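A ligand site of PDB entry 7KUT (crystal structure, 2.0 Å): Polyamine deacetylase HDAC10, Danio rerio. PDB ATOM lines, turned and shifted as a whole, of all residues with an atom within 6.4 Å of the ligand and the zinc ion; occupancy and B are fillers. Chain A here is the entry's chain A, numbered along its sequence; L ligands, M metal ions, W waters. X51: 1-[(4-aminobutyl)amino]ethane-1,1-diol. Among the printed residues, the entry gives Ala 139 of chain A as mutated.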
ATOM      1  N   GLU A  26      18.633 -21.902 -24.426  1.00  0.00           N
ATOM      2  CA  GLU A  26      19.717 -22.864 -24.528  1.00  0.00           C
ATOM      3  C   GLU A  26      20.579 -22.626 -25.762  1.00  0.00           C
ATOM      4  O   GLU A  26      21.808 -22.721 -25.688  1.00  0.00           O
ATOM      5  CB  GLU A  26      19.136 -24.283 -24.550  1.00  0.00           C
ATOM      6  CG  GLU A  26      19.504 -25.119 -23.365  1.00  0.00           C
ATOM      7  CD  GLU A  26      19.421 -26.600 -23.658  1.00  0.00           C
ATOM      8  OE1 GLU A  26      18.345 -27.061 -24.107  1.00  0.00           O
ATOM      9  OE2 GLU A  26      20.439 -27.296 -23.446  1.00  0.00           O
ATOM     10  N   CYS A  27      19.966 -22.321 -26.918  1.00  0.00           N
ATOM     11  CA  CYS A  27      20.720 -22.229 -28.168  1.00  0.00           C
ATOM     12  C   CYS A  27      20.967 -20.805 -28.653  1.00  0.00           C
ATOM     13  O   CYS A  27      21.728 -20.628 -29.611  1.00  0.00           O
ATOM     14  CB  CYS A  27      20.019 -22.998 -29.295  1.00  0.00           C
ATOM     15  SG  CYS A  27      19.637 -24.725 -28.961  1.00  0.00           S
ATOM     16  N   ILE A  29      22.898 -18.588 -27.854  1.00  0.00           N
ATOM     17  CA  ILE A  29      24.294 -18.143 -27.875  1.00  0.00           C
ATOM     18  C   ILE A  29      25.006 -18.502 -29.171  1.00  0.00           C
ATOM     19  O   ILE A  29      26.055 -17.914 -29.480  1.00  0.00           O
ATOM     20  CB  ILE A  29      25.125 -18.770 -26.737  1.00  0.00           C
ATOM     21  CG1 ILE A  29      24.996 -20.296 -26.802  1.00  0.00           C
ATOM     22  CG2 ILE A  29      24.712 -18.212 -25.398  1.00  0.00           C
ATOM     23  CD1 ILE A  29      25.928 -21.033 -25.849  1.00  0.00           C
ATOM     24  N   ASN A  95      18.943 -32.876 -28.488  1.00  0.00           N
ATOM     25  CA  ASN A  95      19.314 -32.121 -27.297  1.00  0.00           C
ATOM     26  C   ASN A  95      20.203 -30.933 -27.655  1.00  0.00           C
ATOM     27  O   ASN A  95      21.305 -31.115 -28.196  1.00  0.00           O
ATOM     28  CB  ASN A  95      20.017 -33.027 -26.291  1.00  0.00           C
ATOM     29  CG  ASN A  95      19.092 -34.083 -25.723  1.00  0.00           C
ATOM     30  OD1 ASN A  95      17.925 -33.821 -25.460  1.00  0.00           O
ATOM     31  ND2 ASN A  95      19.615 -35.288 -25.552  1.00  0.00           N
ATOM     32  N   ALA A  96      19.729 -29.724 -27.349  1.00  0.00           N
ATOM     33  CA  ALA A  96      20.500 -28.484 -27.495  1.00  0.00           C
ATOM     34  C   ALA A  96      20.947 -28.236 -28.938  1.00  0.00           C
ATOM     35  O   ALA A  96      22.130 -28.014 -29.228  1.00  0.00           O
ATOM     36  CB  ALA A  96      21.703 -28.478 -26.531  1.00  0.00           C
ATOM     37  N   PRO A 136      29.238 -26.277 -35.623  1.00  0.00           N
ATOM     38  CA  PRO A 136      30.324 -27.081 -35.041  1.00  0.00           C
ATOM     39  C   PRO A 136      29.979 -28.561 -35.143  1.00  0.00           C
ATOM     40  O   PRO A 136      28.900 -28.951 -35.597  1.00  0.00           O
ATOM     41  CB  PRO A 136      30.400 -26.606 -33.593  1.00  0.00           C
ATOM     42  CG  PRO A 136      29.015 -26.110 -33.274  1.00  0.00           C
ATOM     43  CD  PRO A 136      28.497 -25.523 -34.594  1.00  0.00           C
ATOM     44  N   GLY A 137      30.941 -29.405 -34.768  1.00  0.00           N
ATOM     45  CA  GLY A 137      30.735 -30.826 -35.019  1.00  0.00           C
ATOM     46  C   GLY A 137      30.933 -31.823 -33.888  1.00  0.00           C
ATOM     47  O   GLY A 137      30.287 -32.875 -33.894  1.00  0.00           O
ATOM     48  N   HIS A 138      31.779 -31.509 -32.881  1.00  0.00           N
ATOM     49  CA  HIS A 138      32.342 -32.575 -32.038  1.00  0.00           C
ATOM     50  C   HIS A 138      31.296 -33.284 -31.164  1.00  0.00           C
ATOM     51  O   HIS A 138      31.543 -34.415 -30.725  1.00  0.00           O
ATOM     52  CB  HIS A 138      33.518 -32.038 -31.182  1.00  0.00           C
ATOM     53  CG  HIS A 138      33.113 -31.142 -30.050  1.00  0.00           C
ATOM     54  ND1 HIS A 138      33.878 -31.028 -28.898  1.00  0.00           N
ATOM     55  CD2 HIS A 138      32.063 -30.302 -29.890  1.00  0.00           C
ATOM     56  CE1 HIS A 138      33.306 -30.163 -28.077  1.00  0.00           C
ATOM     57  NE2 HIS A 138      32.202 -29.709 -28.654  1.00  0.00           N
ATOM     58  N   ALA A 139      30.130 -32.686 -30.955  1.00  0.00           N
ATOM     59  CA  ALA A 139      29.084 -33.348 -30.188  1.00  0.00           C
ATOM     60  C   ALA A 139      28.134 -34.193 -31.025  1.00  0.00           C
ATOM     61  O   ALA A 139      27.369 -34.979 -30.443  1.00  0.00           O
ATOM     62  CB  ALA A 139      28.244 -32.313 -29.420  1.00  0.00           C
ATOM     63  N   ASN A 146      23.402 -32.835 -31.883  1.00  0.00           N
ATOM     64  CA  ASN A 146      23.565 -32.622 -30.452  1.00  0.00           C
ATOM     65  C   ASN A 146      24.431 -31.390 -30.223  1.00  0.00           C
ATOM     66  O   ASN A 146      25.452 -31.220 -30.890  1.00  0.00           O
ATOM     67  CB  ASN A 146      24.192 -33.852 -29.793  1.00  0.00           C
ATOM     68  CG  ASN A 146      24.213 -33.768 -28.295  1.00  0.00           C
ATOM     69  OD1 ASN A 146      25.199 -33.320 -27.713  1.00  0.00           O
ATOM     70  ND2 ASN A 146      23.138 -34.204 -27.656  1.00  0.00           N
ATOM     71  N   GLY A 147      24.016 -30.553 -29.280  1.00  0.00           N
ATOM     72  CA  GLY A 147      24.860 -29.456 -28.834  1.00  0.00           C
ATOM     73  C   GLY A 147      25.319 -28.527 -29.943  1.00  0.00           C
ATOM     74  O   GLY A 147      26.521 -28.283 -30.086  1.00  0.00           O
ATOM     75  N   PHE A 148      24.370 -28.019 -30.729  1.00  0.00           N
ATOM     76  CA  PHE A 148      24.565 -27.151 -31.888  1.00  0.00           C
ATOM     77  C   PHE A 148      25.270 -27.837 -33.043  1.00  0.00           C
ATOM     78  O   PHE A 148      25.517 -27.186 -34.066  1.00  0.00           O
ATOM     79  CB  PHE A 148      25.355 -25.863 -31.574  1.00  0.00           C
ATOM     80  CG  PHE A 148      25.027 -25.220 -30.249  1.00  0.00           C
ATOM     81  CD1 PHE A 148      23.726 -25.195 -29.785  1.00  0.00           C
ATOM     82  CD2 PHE A 148      26.019 -24.594 -29.498  1.00  0.00           C
ATOM     83  CE1 PHE A 148      23.425 -24.592 -28.561  1.00  0.00           C
ATOM     84  CE2 PHE A 148      25.708 -23.982 -28.305  1.00  0.00           C
ATOM     85  CZ  PHE A 148      24.413 -23.985 -27.842  1.00  0.00           C
ATOM     86  N   CYS A 149      25.596 -29.130 -32.930  1.00  0.00           N
ATOM     87  CA  CYS A 149      26.322 -29.855 -33.969  1.00  0.00           C
ATOM     88  C   CYS A 149      25.400 -30.746 -34.806  1.00  0.00           C
ATOM     89  O   CYS A 149      24.546 -31.452 -34.259  1.00  0.00           O
ATOM     90  CB  CYS A 149      27.432 -30.698 -33.347  1.00  0.00           C
ATOM     91  SG  CYS A 149      28.581 -29.779 -32.286  1.00  0.00           S
ATOM     92  N   ASP A 176      37.882 -27.409 -26.781  1.00  0.00           N
ATOM     93  CA  ASP A 176      36.571 -26.868 -26.463  1.00  0.00           C
ATOM     94  C   ASP A 176      36.251 -27.181 -25.008  1.00  0.00           C
ATOM     95  O   ASP A 176      36.745 -28.160 -24.449  1.00  0.00           O
ATOM     96  CB  ASP A 176      35.529 -27.500 -27.403  1.00  0.00           C
ATOM     97  CG  ASP A 176      34.179 -26.827 -27.344  1.00  0.00           C
ATOM     98  OD1 ASP A 176      33.869 -26.046 -28.267  1.00  0.00           O
ATOM     99  OD2 ASP A 176      33.404 -27.075 -26.385  1.00  0.00           O
ATOM    100  N   VAL A 177      35.448 -26.323 -24.372  1.00  0.00           N
ATOM    101  CA  VAL A 177      35.153 -26.501 -22.952  1.00  0.00           C
ATOM    102  C   VAL A 177      34.130 -27.604 -22.702  1.00  0.00           C
ATOM    103  O   VAL A 177      33.907 -27.989 -21.542  1.00  0.00           O
ATOM    104  CB  VAL A 177      34.670 -25.178 -22.317  1.00  0.00           C
ATOM    105  CG1 VAL A 177      33.153 -24.995 -22.512  1.00  0.00           C
ATOM    106  CG2 VAL A 177      35.084 -25.097 -20.833  1.00  0.00           C
ATOM    107  N   HIS A 178      33.493 -28.113 -23.754  1.00  0.00           N
ATOM    108  CA  HIS A 178      32.557 -29.222 -23.668  1.00  0.00           C
ATOM    109  C   HIS A 178      33.252 -30.492 -24.153  1.00  0.00           C
ATOM    110  O   HIS A 178      34.126 -30.444 -25.017  1.00  0.00           O
ATOM    111  CB  HIS A 178      31.302 -28.961 -24.524  1.00  0.00           C
ATOM    112  CG  HIS A 178      30.516 -27.753 -24.105  1.00  0.00           C
ATOM    113  ND1 HIS A 178      30.670 -26.518 -24.687  1.00  0.00           N
ATOM    114  CD2 HIS A 178      29.521 -27.611 -23.197  1.00  0.00           C
ATOM    115  CE1 HIS A 178      29.828 -25.659 -24.148  1.00  0.00           C
ATOM    116  NE2 HIS A 178      29.115 -26.293 -23.237  1.00  0.00           N
ATOM    117  N   HIS A 179      32.846 -31.631 -23.583  1.00  0.00           N
ATOM    118  CA  HIS A 179      33.299 -32.928 -24.084  1.00  0.00           C
ATOM    119  C   HIS A 179      32.828 -33.128 -25.528  1.00  0.00           C
ATOM    120  O   HIS A 179      31.686 -32.819 -25.873  1.00  0.00           O
ATOM    121  CB  HIS A 179      32.743 -34.047 -23.207  1.00  0.00           C
ATOM    122  CG  HIS A 179      33.325 -35.397 -23.487  1.00  0.00           C
ATOM    123  ND1 HIS A 179      32.575 -36.549 -23.451  1.00  0.00           N
ATOM    124  CD2 HIS A 179      34.587 -35.772 -23.781  1.00  0.00           C
ATOM    125  CE1 HIS A 179      33.348 -37.584 -23.739  1.00  0.00           C
ATOM    126  NE2 HIS A 179      34.573 -37.135 -23.940  1.00  0.00           N
ATOM    127  N   TRP A 207      26.653 -29.988 -18.825  1.00  0.00           N
ATOM    128  CA  TRP A 207      26.363 -30.506 -20.155  1.00  0.00           C
ATOM    129  C   TRP A 207      27.625 -31.072 -20.816  1.00  0.00           C
ATOM    130  O   TRP A 207      28.677 -30.427 -20.783  1.00  0.00           O
ATOM    131  CB  TRP A 207      25.750 -29.388 -21.008  1.00  0.00           C
ATOM    132  CG  TRP A 207      25.057 -29.924 -22.203  1.00  0.00           C
ATOM    133  CD1 TRP A 207      23.742 -30.268 -22.316  1.00  0.00           C
ATOM    134  CD2 TRP A 207      25.667 -30.267 -23.452  1.00  0.00           C
ATOM    135  NE1 TRP A 207      23.490 -30.790 -23.567  1.00  0.00           N
ATOM    136  CE2 TRP A 207      24.662 -30.804 -24.275  1.00  0.00           C
ATOM    137  CE3 TRP A 207      26.973 -30.175 -23.942  1.00  0.00           C
ATOM    138  CZ2 TRP A 207      24.912 -31.221 -25.578  1.00  0.00           C
ATOM    139  CZ3 TRP A 207      27.227 -30.599 -25.238  1.00  0.00           C
ATOM    140  CH2 TRP A 207      26.200 -31.117 -26.045  1.00  0.00           C
ATOM    141  N   GLY A 267      37.524 -25.290 -29.735  1.00  0.00           N
ATOM    142  CA  GLY A 267      36.489 -24.473 -29.150  1.00  0.00           C
ATOM    143  C   GLY A 267      37.115 -23.470 -28.207  1.00  0.00           C
ATOM    144  O   GLY A 267      37.890 -23.840 -27.318  1.00  0.00           O
ATOM    145  N   ASP A 269      35.292 -21.519 -26.317  1.00  0.00           N
ATOM    146  CA  ASP A 269      34.509 -21.343 -25.108  1.00  0.00           C
ATOM    147  C   ASP A 269      35.263 -21.802 -23.869  1.00  0.00           C
ATOM    148  O   ASP A 269      34.721 -21.742 -22.767  1.00  0.00           O
ATOM    149  CB  ASP A 269      33.154 -22.057 -25.223  1.00  0.00           C
ATOM    150  CG  ASP A 269      33.260 -23.533 -25.656  1.00  0.00           C
ATOM    151  OD1 ASP A 269      34.371 -24.115 -25.663  1.00  0.00           O
ATOM    152  OD2 ASP A 269      32.179 -24.094 -25.970  1.00  0.00           O
ATOM    153  N   GLU A 276      29.419 -20.015 -21.385  1.00  0.00           N
ATOM    154  CA  GLU A 276      29.276 -21.449 -21.171  1.00  0.00           C
ATOM    155  C   GLU A 276      30.413 -22.032 -20.359  1.00  0.00           C
ATOM    156  O   GLU A 276      30.177 -22.847 -19.457  1.00  0.00           O
ATOM    157  CB  GLU A 276      29.201 -22.181 -22.519  1.00  0.00           C
ATOM    158  CG  GLU A 276      27.844 -22.183 -23.142  1.00  0.00           C
ATOM    159  CD  GLU A 276      26.883 -23.060 -22.377  1.00  0.00           C
ATOM    160  OE1 GLU A 276      27.038 -24.309 -22.422  1.00  0.00           O
ATOM    161  OE2 GLU A 276      25.968 -22.502 -21.736  1.00  0.00           O
ATOM    162  N   GLU A 306      35.219 -25.141 -33.269  1.00  0.00           N
ATOM    163  CA  GLU A 306      34.035 -25.723 -32.645  1.00  0.00           C
ATOM    164  C   GLU A 306      33.237 -24.608 -31.975  1.00  0.00           C
ATOM    165  O   GLU A 306      32.585 -23.814 -32.679  1.00  0.00           O
ATOM    166  CB  GLU A 306      34.437 -26.856 -31.679  1.00  0.00           C
ATOM    167  CG  GLU A 306      35.254 -27.933 -32.368  1.00  0.00           C
ATOM    168  CD  GLU A 306      34.389 -29.067 -32.960  1.00  0.00           C
ATOM    169  OE1 GLU A 306      33.134 -28.968 -32.939  1.00  0.00           O
ATOM    170  OE2 GLU A 306      34.960 -30.080 -33.423  1.00  0.00           O
ATOM    171  N   GLY A 307      33.227 -24.513 -30.646  1.00  0.00           N
ATOM    172  CA  GLY A 307      32.458 -23.503 -29.944  1.00  0.00           C
ATOM    173  C   GLY A 307      33.246 -22.221 -29.663  1.00  0.00           C
ATOM    174  O   GLY A 307      34.330 -21.992 -30.205  1.00  0.00           O
ATOM    175  N   GLY A 308      32.658 -21.364 -28.810  1.00  0.00           N
ATOM    176  CA  GLY A 308      33.240 -20.077 -28.414  1.00  0.00           C
ATOM    177  C   GLY A 308      32.249 -18.941 -28.565  1.00  0.00           C
ATOM    178  O   GLY A 308      31.923 -18.566 -29.691  1.00  0.00           O
ATOM    179  N   TYR A 309      31.725 -18.405 -27.453  1.00  0.00           N
ATOM    180  CA  TYR A 309      30.481 -17.645 -27.511  1.00  0.00           C
ATOM    181  C   TYR A 309      30.574 -16.214 -26.999  1.00  0.00           C
ATOM    182  O   TYR A 309      29.598 -15.481 -27.139  1.00  0.00           O
ATOM    183  CB  TYR A 309      29.360 -18.379 -26.738  1.00  0.00           C
ATOM    184  CG  TYR A 309      29.241 -19.774 -27.260  1.00  0.00           C
ATOM    185  CD1 TYR A 309      28.593 -20.020 -28.458  1.00  0.00           C
ATOM    186  CD2 TYR A 309      29.841 -20.844 -26.595  1.00  0.00           C
ATOM    187  CE1 TYR A 309      28.525 -21.303 -28.978  1.00  0.00           C
ATOM    188  CE2 TYR A 309      29.764 -22.113 -27.082  1.00  0.00           C
ATOM    189  CZ  TYR A 309      29.105 -22.351 -28.281  1.00  0.00           C
ATOM    190  OH  TYR A 309      29.039 -23.617 -28.786  1.00  0.00           O
HETATM  191  C01 X51 L   1      30.090 -26.876 -29.775  1.00  0.00           C
HETATM  192  C02 X51 L   1      29.861 -26.904 -28.250  1.00  0.00           C
HETATM  193  C06 X51 L   1      27.846 -26.429 -26.931  1.00  0.00           C
HETATM  194  C07 X51 L   1      26.520 -27.064 -26.469  1.00  0.00           C
HETATM  195  C08 X51 L   1      25.848 -26.232 -25.376  1.00  0.00           C
HETATM  196  C09 X51 L   1      24.587 -26.904 -24.807  1.00  0.00           C
HETATM  197  N05 X51 L   1      28.462 -27.240 -27.971  1.00  0.00           N
HETATM  198  N10 X51 L   1      23.935 -26.013 -23.866  1.00  0.00           N
HETATM  199  O03 X51 L   1      30.643 -27.913 -27.698  1.00  0.00           O
HETATM  200  O04 X51 L   1      30.252 -25.664 -27.755  1.00  0.00           O
HETATM  201 ZN    ZN M   1      31.868 -26.040 -26.440  1.00  0.00          ZN
HETATM  202  O   HOH W   1      23.881 -22.726 -23.667  1.00  0.00           O
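Along chain A the residues within 4 Å of the zinc ion span positions 176 to 269.
The nearest printed residue that does not touch the zinc ion is Val 177 (4.1 Å).
Water W1 lies within hydrogen-bond range of OE2 of Glu 276, O of Glu 26 and N10 of the ligand.
A ring nitrogen (NE2) of His 138 lies close to an oxygen (O03) of the ligand (2.6 Å).
The side-chain hydroxyl of Tyr 309 lies close to an oxygen (O04) of the ligand, 2.6 Å away.
A nitrogen (N05) of the ligand lies within hydrogen-bond range of the backbone carbonyl oxygen of Gly 147 (3.1 Å).
The side-chain carboxylate (OE1) of Glu 276 is in salt-bridge range of a nitrogen (N10) of the ligand, at 3.8 Å.
A nitrogen (N10) of the ligand is in salt-bridge range of the side-chain carboxylate of Glu 26, at 3.7 Å.
Merely in contact with the ligand: Ala 96 (3.7 Å), Pro 136 (3.7 Å), Phe 148 (3.5 Å), Trp 207 (3.8 Å) and Gly 307 (3.8 Å).
Hydrophobic or aromatic side chains within 4 Å of the ligand: Ala 96, Pro 136, His 138, Phe 148, His 178, Trp 207 and Tyr 309.
Of the 25 residues printed, 13 come within 4 Å of the ligand.
Along chain A the residues within 4 Å of the ligand span positions 26 to 309.
The nearest printed residue that does not touch the ligand is Cys 149 (4.1 Å).
OD1 of Asp 176 lies within hydrogen-bond range of N of Gly 307 (2.9 Å).
OD1 of Asp 269 sits at hydrogen-bond distance from N of Val 177 (2.8 Å).
N of His 138 lies within hydrogen-bond range of OE1 of Glu 306 (2.9 Å).
The backbone NH (N) of Gly 147 lies close to the backbone carbonyl oxygen (O) of Ala 96 (3.2 Å).
The backbone carbonyl oxygen of Gly 147 sits at hydrogen-bond distance from the side-chain sulfur of Cys 149 (3.4 Å).
N of Gly 147 is in hydrogen-bond range of O of Asn 95, at 3.0 Å.
The backbone NH of Phe 148 is in hydrogen-bond range of the backbone carbonyl oxygen of Ala 96, 2.7 Å away.
O of Pro 136 lies close to SG of Cys 149.
The zinc ion is bound by the side-chain carboxylate (OD2) of Asp 176 (1.9 Å), the side-chain carboxylate (OD2) of Asp 269 (2.0 Å), an oxygen (O04) of the ligand (2.1 Å), a ring nitrogen (ND1) of His 178 (2.2 Å) and an oxygen (O03) of the ligand (2.6 Å).
The zinc ion has five donor atoms within binding distance.
Slightly farther from the zinc ion lies OD1 of Asp 176 (2.7 Å).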
